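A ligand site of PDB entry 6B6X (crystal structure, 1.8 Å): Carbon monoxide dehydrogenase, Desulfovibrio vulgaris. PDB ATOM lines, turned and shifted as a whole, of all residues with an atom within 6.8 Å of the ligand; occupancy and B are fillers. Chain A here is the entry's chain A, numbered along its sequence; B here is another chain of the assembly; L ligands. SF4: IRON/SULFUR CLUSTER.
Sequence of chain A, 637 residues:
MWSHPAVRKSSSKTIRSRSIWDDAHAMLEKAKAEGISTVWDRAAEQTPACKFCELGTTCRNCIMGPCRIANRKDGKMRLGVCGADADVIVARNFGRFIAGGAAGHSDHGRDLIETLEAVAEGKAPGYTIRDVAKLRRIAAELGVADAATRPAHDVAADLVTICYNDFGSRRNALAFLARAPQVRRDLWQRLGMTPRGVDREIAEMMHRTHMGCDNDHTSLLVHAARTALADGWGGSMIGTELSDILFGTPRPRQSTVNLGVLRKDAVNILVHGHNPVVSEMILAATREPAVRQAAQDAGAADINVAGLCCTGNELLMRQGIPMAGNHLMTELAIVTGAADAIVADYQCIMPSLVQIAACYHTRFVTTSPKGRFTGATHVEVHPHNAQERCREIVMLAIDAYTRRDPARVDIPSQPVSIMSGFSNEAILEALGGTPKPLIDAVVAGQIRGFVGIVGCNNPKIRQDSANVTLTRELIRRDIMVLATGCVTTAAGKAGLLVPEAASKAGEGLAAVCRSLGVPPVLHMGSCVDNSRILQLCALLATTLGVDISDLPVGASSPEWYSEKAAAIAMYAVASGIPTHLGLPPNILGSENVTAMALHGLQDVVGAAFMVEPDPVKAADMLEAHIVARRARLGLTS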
ATOM      1  N   THR A  58       5.746  35.159  -3.986  1.00  0.00           N
ATOM      2  CA  THR A  58       4.901  33.981  -3.925  1.00  0.00           C
ATOM      3  C   THR A  58       4.358  33.737  -5.322  1.00  0.00           C
ATOM      4  O   THR A  58       4.139  34.677  -6.082  1.00  0.00           O
ATOM      5  CB  THR A  58       3.761  34.146  -2.899  1.00  0.00           C
ATOM      6  OG1 THR A  58       2.854  33.038  -2.986  1.00  0.00           O
ATOM      7  CG2 THR A  58       2.999  35.448  -3.142  1.00  0.00           C
ATOM      8  N   CYS A  59       4.172  32.470  -5.669  1.00  0.00           N
ATOM      9  CA  CYS A  59       3.715  32.143  -7.013  1.00  0.00           C
ATOM     10  C   CYS A  59       2.701  31.009  -6.936  1.00  0.00           C
ATOM     11  O   CYS A  59       2.915  30.029  -6.208  1.00  0.00           O
ATOM     12  CB  CYS A  59       4.891  31.748  -7.922  1.00  0.00           C
ATOM     13  SG  CYS A  59       4.446  31.445  -9.651  1.00  0.00           S
ATOM     14  N   ARG A  60       1.604  31.144  -7.680  1.00  0.00           N
ATOM     15  CA  ARG A  60       0.571  30.122  -7.753  1.00  0.00           C
ATOM     16  C   ARG A  60       0.249  29.765  -9.199  1.00  0.00           C
ATOM     17  O   ARG A  60      -0.885  29.390  -9.516  1.00  0.00           O
ATOM     18  CB  ARG A  60      -0.702  30.577  -7.039  1.00  0.00           C
ATOM     19  CG  ARG A  60      -0.486  31.109  -5.635  1.00  0.00           C
ATOM     20  CD  ARG A  60      -1.797  31.542  -4.989  1.00  0.00           C
ATOM     21  NE  ARG A  60      -2.123  32.944  -5.230  1.00  0.00           N
ATOM     22  CZ  ARG A  60      -3.030  33.365  -6.107  1.00  0.00           C
ATOM     23  NH1 ARG A  60      -3.701  32.485  -6.842  1.00  0.00           N
ATOM     24  NH2 ARG A  60      -3.265  34.664  -6.247  1.00  0.00           N
ATOM     25  N   ASN A  61       1.237  29.861 -10.091  1.00  0.00           N
ATOM     26  CA  ASN A  61       0.983  29.722 -11.517  1.00  0.00           C
ATOM     27  C   ASN A  61       0.992  28.280 -12.006  1.00  0.00           C
ATOM     28  O   ASN A  61       0.686  28.035 -13.171  1.00  0.00           O
ATOM     29  CB  ASN A  61       2.006  30.541 -12.321  1.00  0.00           C
ATOM     30  CG  ASN A  61       1.760  32.049 -12.229  1.00  0.00           C
ATOM     31  OD1 ASN A  61       2.423  32.840 -12.897  1.00  0.00           O
ATOM     32  ND2 ASN A  61       0.816  32.447 -11.392  1.00  0.00           N
ATOM     33  N   CYS A  62       1.330  27.309 -11.152  1.00  0.00           N
ATOM     34  CA  CYS A  62       1.157  25.901 -11.504  1.00  0.00           C
ATOM     35  C   CYS A  62       1.027  25.112 -10.208  1.00  0.00           C
ATOM     36  O   CYS A  62       1.251  25.635  -9.119  1.00  0.00           O
ATOM     37  CB  CYS A  62       2.317  25.396 -12.369  1.00  0.00           C
ATOM     38  SG  CYS A  62       3.800  24.935 -11.451  1.00  0.00           S
ATOM     39  N   ILE A  63       0.650  23.836 -10.328  1.00  0.00           N
ATOM     40  CA  ILE A  63       0.469  23.008  -9.140  1.00  0.00           C
ATOM     41  C   ILE A  63       1.666  22.078  -8.913  1.00  0.00           C
ATOM     42  O   ILE A  63       1.562  21.108  -8.163  1.00  0.00           O
ATOM     43  CB  ILE A  63      -0.854  22.226  -9.144  1.00  0.00           C
ATOM     44  CG1 ILE A  63      -0.868  21.108 -10.190  1.00  0.00           C
ATOM     45  CG2 ILE A  63      -2.040  23.178  -9.290  1.00  0.00           C
ATOM     46  CD1 ILE A  63      -1.678  19.898  -9.761  1.00  0.00           C
ATOM     47  N   MET A  64       2.817  22.362  -9.547  1.00  0.00           N
ATOM     48  CA  MET A  64       4.059  21.962  -8.885  1.00  0.00           C
ATOM     49  C   MET A  64       4.230  22.776  -7.613  1.00  0.00           C
ATOM     50  O   MET A  64       4.754  22.265  -6.613  1.00  0.00           O
ATOM     51  CB  MET A  64       5.263  22.136  -9.809  1.00  0.00           C
ATOM     52  CG  MET A  64       5.262  21.224 -11.032  1.00  0.00           C
ATOM     53  SD  MET A  64       6.937  20.908 -11.625  1.00  0.00           S
ATOM     54  CE  MET A  64       7.489  22.566 -12.021  1.00  0.00           C
ATOM     55  N   GLY A  65       3.790  24.032  -7.629  1.00  0.00           N
ATOM     56  CA  GLY A  65       3.715  24.849  -6.445  1.00  0.00           C
ATOM     57  C   GLY A  65       2.440  24.583  -5.672  1.00  0.00           C
ATOM     58  O   GLY A  65       1.847  23.499  -5.757  1.00  0.00           O
ATOM     59  N   PRO A  66       1.952  25.584  -4.914  1.00  0.00           N
ATOM     60  CA  PRO A  66       2.438  26.973  -4.889  1.00  0.00           C
ATOM     61  C   PRO A  66       3.780  27.128  -4.183  1.00  0.00           C
ATOM     62  O   PRO A  66       4.150  26.280  -3.363  1.00  0.00           O
ATOM     63  CB  PRO A  66       1.337  27.712  -4.123  1.00  0.00           C
ATOM     64  CG  PRO A  66       0.769  26.679  -3.215  1.00  0.00           C
ATOM     65  CD  PRO A  66       0.817  25.382  -4.001  1.00  0.00           C
ATOM     66  N   CYS A  67       4.493  28.215  -4.488  1.00  0.00           N
ATOM     67  CA  CYS A  67       5.852  28.412  -4.033  1.00  0.00           C
ATOM     68  C   CYS A  67       5.988  29.748  -3.309  1.00  0.00           C
ATOM     69  O   CYS A  67       5.299  30.715  -3.640  1.00  0.00           O
ATOM     70  CB  CYS A  67       6.854  28.381  -5.191  1.00  0.00           C
ATOM     71  SG  CYS A  67       6.801  26.891  -6.193  1.00  0.00           S
ATOM     72  N   ARG A  68       6.901  29.781  -2.343  1.00  0.00           N
ATOM     73  CA  ARG A  68       7.288  31.003  -1.662  1.00  0.00           C
ATOM     74  C   ARG A  68       8.802  31.133  -1.710  1.00  0.00           C
ATOM     75  O   ARG A  68       9.524  30.136  -1.617  1.00  0.00           O
ATOM     76  CB  ARG A  68       6.789  31.008  -0.209  1.00  0.00           C
ATOM     77  CG  ARG A  68       5.280  31.233  -0.081  1.00  0.00           C
ATOM     78  CD  ARG A  68       4.765  30.751   1.262  1.00  0.00           C
ATOM     79  NE  ARG A  68       4.956  29.311   1.397  1.00  0.00           N
ATOM     80  CZ  ARG A  68       4.915  28.654   2.550  1.00  0.00           C
ATOM     81  NH1 ARG A  68       4.675  29.307   3.681  1.00  0.00           N
ATOM     82  NH2 ARG A  68       5.111  27.344   2.564  1.00  0.00           N
ATOM     83  N   ILE A  69       9.298  32.361  -1.872  1.00  0.00           N
ATOM     84  CA  ILE A  69      10.718  32.640  -1.986  1.00  0.00           C
ATOM     85  C   ILE A  69      11.182  33.425  -0.765  1.00  0.00           C
ATOM     86  O   ILE A  69      10.528  34.379  -0.343  1.00  0.00           O
ATOM     87  CB  ILE A  69      11.063  33.410  -3.271  1.00  0.00           C
ATOM     88  CG1 ILE A  69      10.473  32.697  -4.479  1.00  0.00           C
ATOM     89  CG2 ILE A  69      12.571  33.557  -3.418  1.00  0.00           C
ATOM     90  CD1 ILE A  69      11.050  31.318  -4.715  1.00  0.00           C
ATOM     91  N   LEU A  79      14.444  29.310  -4.891  1.00  0.00           N
ATOM     92  CA  LEU A  79      13.842  29.102  -6.196  1.00  0.00           C
ATOM     93  C   LEU A  79      12.506  28.398  -6.029  1.00  0.00           C
ATOM     94  O   LEU A  79      12.295  27.646  -5.073  1.00  0.00           O
ATOM     95  CB  LEU A  79      14.751  28.265  -7.117  1.00  0.00           C
ATOM     96  CG  LEU A  79      16.191  28.751  -7.246  1.00  0.00           C
ATOM     97  CD1 LEU A  79      17.046  27.776  -8.030  1.00  0.00           C
ATOM     98  CD2 LEU A  79      16.194  30.126  -7.898  1.00  0.00           C
ATOM     99  N   GLY A  80      11.604  28.639  -6.972  1.00  0.00           N
ATOM    100  CA  GLY A  80      10.392  27.840  -7.052  1.00  0.00           C
ATOM    101  C   GLY A  80      10.704  26.434  -7.518  1.00  0.00           C
ATOM    102  O   GLY A  80      11.832  26.100  -7.878  1.00  0.00           O
ATOM    103  N   VAL A  81       9.677  25.582  -7.496  1.00  0.00           N
ATOM    104  CA  VAL A  81       9.890  24.193  -7.897  1.00  0.00           C
ATOM    105  C   VAL A  81      10.428  24.120  -9.321  1.00  0.00           C
ATOM    106  O   VAL A  81      11.276  23.275  -9.627  1.00  0.00           O
ATOM    107  CB  VAL A  81       8.583  23.388  -7.722  1.00  0.00           C
ATOM    108  CG1 VAL A  81       8.768  21.940  -8.174  1.00  0.00           C
ATOM    109  CG2 VAL A  81       8.127  23.436  -6.270  1.00  0.00           C
ATOM    110  N   CYS A  82       9.980  25.016 -10.197  1.00  0.00           N
ATOM    111  CA  CYS A  82      10.454  25.068 -11.571  1.00  0.00           C
ATOM    112  C   CYS A  82      11.844  25.690 -11.702  1.00  0.00           C
ATOM    113  O   CYS A  82      12.426  25.632 -12.796  1.00  0.00           O
ATOM    114  CB  CYS A  82       9.470  25.851 -12.447  1.00  0.00           C
ATOM    115  SG  CYS A  82       9.306  27.606 -12.011  1.00  0.00           S
ATOM    116  N   GLY A  83      12.371  26.304 -10.646  1.00  0.00           N
ATOM    117  CA  GLY A  83      13.671  26.949 -10.701  1.00  0.00           C
ATOM    118  C   GLY A  83      13.623  28.459 -10.839  1.00  0.00           C
ATOM    119  O   GLY A  83      14.683  29.092 -10.874  1.00  0.00           O
ATOM    120  N   ALA A  84      12.430  29.051 -10.923  1.00  0.00           N
ATOM    121  CA  ALA A  84      12.318  30.497 -11.048  1.00  0.00           C
ATOM    122  C   ALA A  84      12.755  31.184  -9.761  1.00  0.00           C
ATOM    123  O   ALA A  84      12.422  30.749  -8.661  1.00  0.00           O
ATOM    124  CB  ALA A  84      10.877  30.886 -11.380  1.00  0.00           C
ATOM    125  N   ILE A  89       9.681  35.649 -10.418  1.00  0.00           N
ATOM    126  CA  ILE A  89       8.357  35.496  -9.800  1.00  0.00           C
ATOM    127  C   ILE A  89       7.722  36.862  -9.568  1.00  0.00           C
ATOM    128  O   ILE A  89       6.546  37.084  -9.889  1.00  0.00           O
ATOM    129  CB  ILE A  89       8.477  34.682  -8.499  1.00  0.00           C
ATOM    130  CG1 ILE A  89       8.717  33.211  -8.850  1.00  0.00           C
ATOM    131  CG2 ILE A  89       7.225  34.882  -7.617  1.00  0.00           C
ATOM    132  CD1 ILE A  89       9.239  32.368  -7.695  1.00  0.00           C
ATOM    133  N   ARG A  92       6.760  38.412 -12.983  1.00  0.00           N
ATOM    134  CA  ARG A  92       5.569  37.782 -13.557  1.00  0.00           C
ATOM    135  C   ARG A  92       4.304  38.230 -12.835  1.00  0.00           C
ATOM    136  O   ARG A  92       3.278  38.483 -13.477  1.00  0.00           O
ATOM    137  CB  ARG A  92       5.691  36.265 -13.512  1.00  0.00           C
ATOM    138  CG  ARG A  92       6.752  35.702 -14.429  1.00  0.00           C
ATOM    139  CD  ARG A  92       6.650  34.189 -14.566  1.00  0.00           C
ATOM    140  NE  ARG A  92       6.704  33.484 -13.277  1.00  0.00           N
ATOM    141  CZ  ARG A  92       7.107  32.227 -13.165  1.00  0.00           C
ATOM    142  NH1 ARG A  92       7.498  31.552 -14.237  1.00  0.00           N
ATOM    143  NH2 ARG A  92       7.135  31.630 -11.975  1.00  0.00           N
ATOM    144  N   THR A 209       3.907  34.604 -18.692  1.00  0.00           N
ATOM    145  CA  THR A 209       3.947  34.348 -17.252  1.00  0.00           C
ATOM    146  C   THR A 209       3.562  32.918 -16.888  1.00  0.00           C
ATOM    147  O   THR A 209       3.591  32.576 -15.697  1.00  0.00           O
ATOM    148  CB  THR A 209       3.056  35.357 -16.521  1.00  0.00           C
ATOM    149  OG1 THR A 209       1.752  35.368 -17.106  1.00  0.00           O
ATOM    150  CG2 THR A 209       3.646  36.763 -16.630  1.00  0.00           C
ATOM    151  N   HIS A 210       3.202  32.082 -17.864  1.00  0.00           N
ATOM    152  CA  HIS A 210       3.090  30.640 -17.649  1.00  0.00           C
ATOM    153  C   HIS A 210       4.459  30.083 -17.261  1.00  0.00           C
ATOM    154  O   HIS A 210       5.498  30.606 -17.667  1.00  0.00           O
ATOM    155  CB  HIS A 210       2.588  29.960 -18.937  1.00  0.00           C
ATOM    156  CG  HIS A 210       2.225  28.513 -18.791  1.00  0.00           C
ATOM    157  ND1 HIS A 210       3.158  27.516 -18.666  1.00  0.00           N
ATOM    158  CD2 HIS A 210       1.012  27.890 -18.775  1.00  0.00           C
ATOM    159  CE1 HIS A 210       2.555  26.352 -18.554  1.00  0.00           C
ATOM    160  NE2 HIS A 210       1.248  26.547 -18.628  1.00  0.00           N
ATOM    161  N   MET A 211       4.450  29.021 -16.440  1.00  0.00           N
ATOM    162  CA  MET A 211       5.700  28.341 -16.087  1.00  0.00           C
ATOM    163  C   MET A 211       6.525  28.101 -17.340  1.00  0.00           C
ATOM    164  O   MET A 211       6.000  27.699 -18.378  1.00  0.00           O
ATOM    165  CB  MET A 211       5.430  26.996 -15.397  1.00  0.00           C
ATOM    166  CG  MET A 211       6.668  26.300 -14.760  1.00  0.00           C
ATOM    167  SD  MET A 211       7.950  25.645 -15.887  1.00  0.00           S
ATOM    168  CE  MET A 211       7.771  23.873 -15.631  1.00  0.00           C
ATOM    169  N   GLY A 212       7.822  28.372 -17.246  1.00  0.00           N
ATOM    170  CA  GLY A 212       8.745  27.999 -18.291  1.00  0.00           C
ATOM    171  C   GLY A 212       8.601  28.736 -19.606  1.00  0.00           C
ATOM    172  O   GLY A 212       8.989  28.193 -20.645  1.00  0.00           O
ATOM    173  N   GLN B  46       9.606  23.266  -0.872  1.00  0.00           N
ATOM    174  CA  GLN B  46       8.339  23.978  -0.927  1.00  0.00           C
ATOM    175  C   GLN B  46       7.194  23.203  -0.285  1.00  0.00           C
ATOM    176  O   GLN B  46       6.036  23.600  -0.421  1.00  0.00           O
ATOM    177  CB  GLN B  46       7.997  24.311  -2.382  1.00  0.00           C
ATOM    178  CG  GLN B  46       8.981  25.290  -3.055  1.00  0.00           C
ATOM    179  CD  GLN B  46       8.915  26.696  -2.460  1.00  0.00           C
ATOM    180  OE1 GLN B  46       7.923  27.076  -1.830  1.00  0.00           O
ATOM    181  NE2 GLN B  46       9.968  27.471  -2.665  1.00  0.00           N
ATOM    182  N   PRO B 351      13.625  27.022 -15.781  1.00  0.00           N
ATOM    183  CA  PRO B 351      14.842  27.840 -15.771  1.00  0.00           C
ATOM    184  C   PRO B 351      15.994  27.193 -15.027  1.00  0.00           C
ATOM    185  O   PRO B 351      17.149  27.610 -15.205  1.00  0.00           O
ATOM    186  CB  PRO B 351      14.389  29.145 -15.083  1.00  0.00           C
ATOM    187  CG  PRO B 351      13.131  28.774 -14.340  1.00  0.00           C
ATOM    188  CD  PRO B 351      12.474  27.719 -15.174  1.00  0.00           C
ATOM    189  N   TYR B 561       0.431  19.320 -14.058  1.00  0.00           N
ATOM    190  CA  TYR B 561       0.945  20.447 -13.281  1.00  0.00           C
ATOM    191  C   TYR B 561       0.555  21.812 -13.840  1.00  0.00           C
ATOM    192  O   TYR B 561       0.363  22.742 -13.047  1.00  0.00           O
ATOM    193  CB  TYR B 561       2.486  20.372 -13.167  1.00  0.00           C
ATOM    194  CG  TYR B 561       3.187  21.236 -14.198  1.00  0.00           C
ATOM    195  CD1 TYR B 561       3.447  22.581 -13.945  1.00  0.00           C
ATOM    196  CD2 TYR B 561       3.549  20.724 -15.434  1.00  0.00           C
ATOM    197  CE1 TYR B 561       4.037  23.390 -14.895  1.00  0.00           C
ATOM    198  CE2 TYR B 561       4.160  21.526 -16.387  1.00  0.00           C
ATOM    199  CZ  TYR B 561       4.387  22.862 -16.110  1.00  0.00           C
ATOM    200  OH  TYR B 561       4.979  23.685 -17.049  1.00  0.00           O
HETATM  201 FE1  SF4 L   1       5.286  29.356  -9.931  1.00  0.00          FE
HETATM  202 FE2  SF4 L   1       6.262  27.405  -8.335  1.00  0.00          FE
HETATM  203 FE3  SF4 L   1       7.367  27.818 -10.825  1.00  0.00          FE
HETATM  204 FE4  SF4 L   1       4.835  26.763 -10.580  1.00  0.00          FE
HETATM  205  S1  SF4 L   1       6.801  25.817  -9.879  1.00  0.00           S
HETATM  206  S2  SF4 L   1       5.495  28.433 -11.992  1.00  0.00           S
HETATM  207  S3  SF4 L   1       4.055  27.841  -8.744  1.00  0.00           S
HETATM  208  S4  SF4 L   1       7.387  29.251  -9.044  1.00  0.00           S
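N of Val 81 lies close to S1 of the ligand.
An iron atom (FE1) of the ligand is bound by the side-chain sulfur (SG) of Cys 59 (2.3 Å).
SG of Cys 67 is bound to FE2 of the ligand (2.3 Å).
The side-chain sulfur (SG) of Cys 62 binds an iron atom (FE4) of the ligand (2.3 Å).
S1 of the ligand lies close to N of Cys 82 (3.3 Å).
NH2 of Arg 92 lies close to S2 of the ligand, at 3.6 Å.
An iron atom (FE3) of the ligand is bound by the side-chain sulfur of Cys 82.
S3 of the ligand sits close to N of Asn 61 (3.7 Å).
S3 of the ligand lies close to N of Cys 62 (3.7 Å).
N of Cys 59 sits at hydrogen-bond distance from O of Cys 67.
The side-chain sulfur (SG) of Cys 67 sits close to the backbone NH (N) of Val 81 (3.4 Å).
The side-chain sulfur (SG) of Cys 59 lies close to the backbone NH (N) of Asn 61.
The side-chain hydroxyl (OH) of Tyr 561 of chain B lies close to the side-chain sulfur (SD) of Met 211 (3.7 Å).
The side-chain sulfur (SG) of Cys 59 lies close to the guanidinium group (NH2) of Arg 92, 3.6 Å away.
SG of Cys 82 sits close to N of Ala 84, 3.6 Å away.
OG1 of Thr 58 lies close to O of Cys 67, at 3.4 Å.
O of Thr 209 sits close to OD1 of Asn 61, 3.0 Å away.
Merely in contact with the ligand: Met 211, Gly 65, Ile 89, Gly 80 and Met 64.
Hydrophobic or aromatic side chains within 4 Å of the ligand: Met 64, Val 81, Ile 89 and Met 211.
12 residues have an atom within 4 Å of the ligand: Cys 59, Asn 61, Cys 62, Met 64, Gly 65, Cys 67, Gly 80, Val 81, Cys 82, Ile 89, Arg 92 and Met 211.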
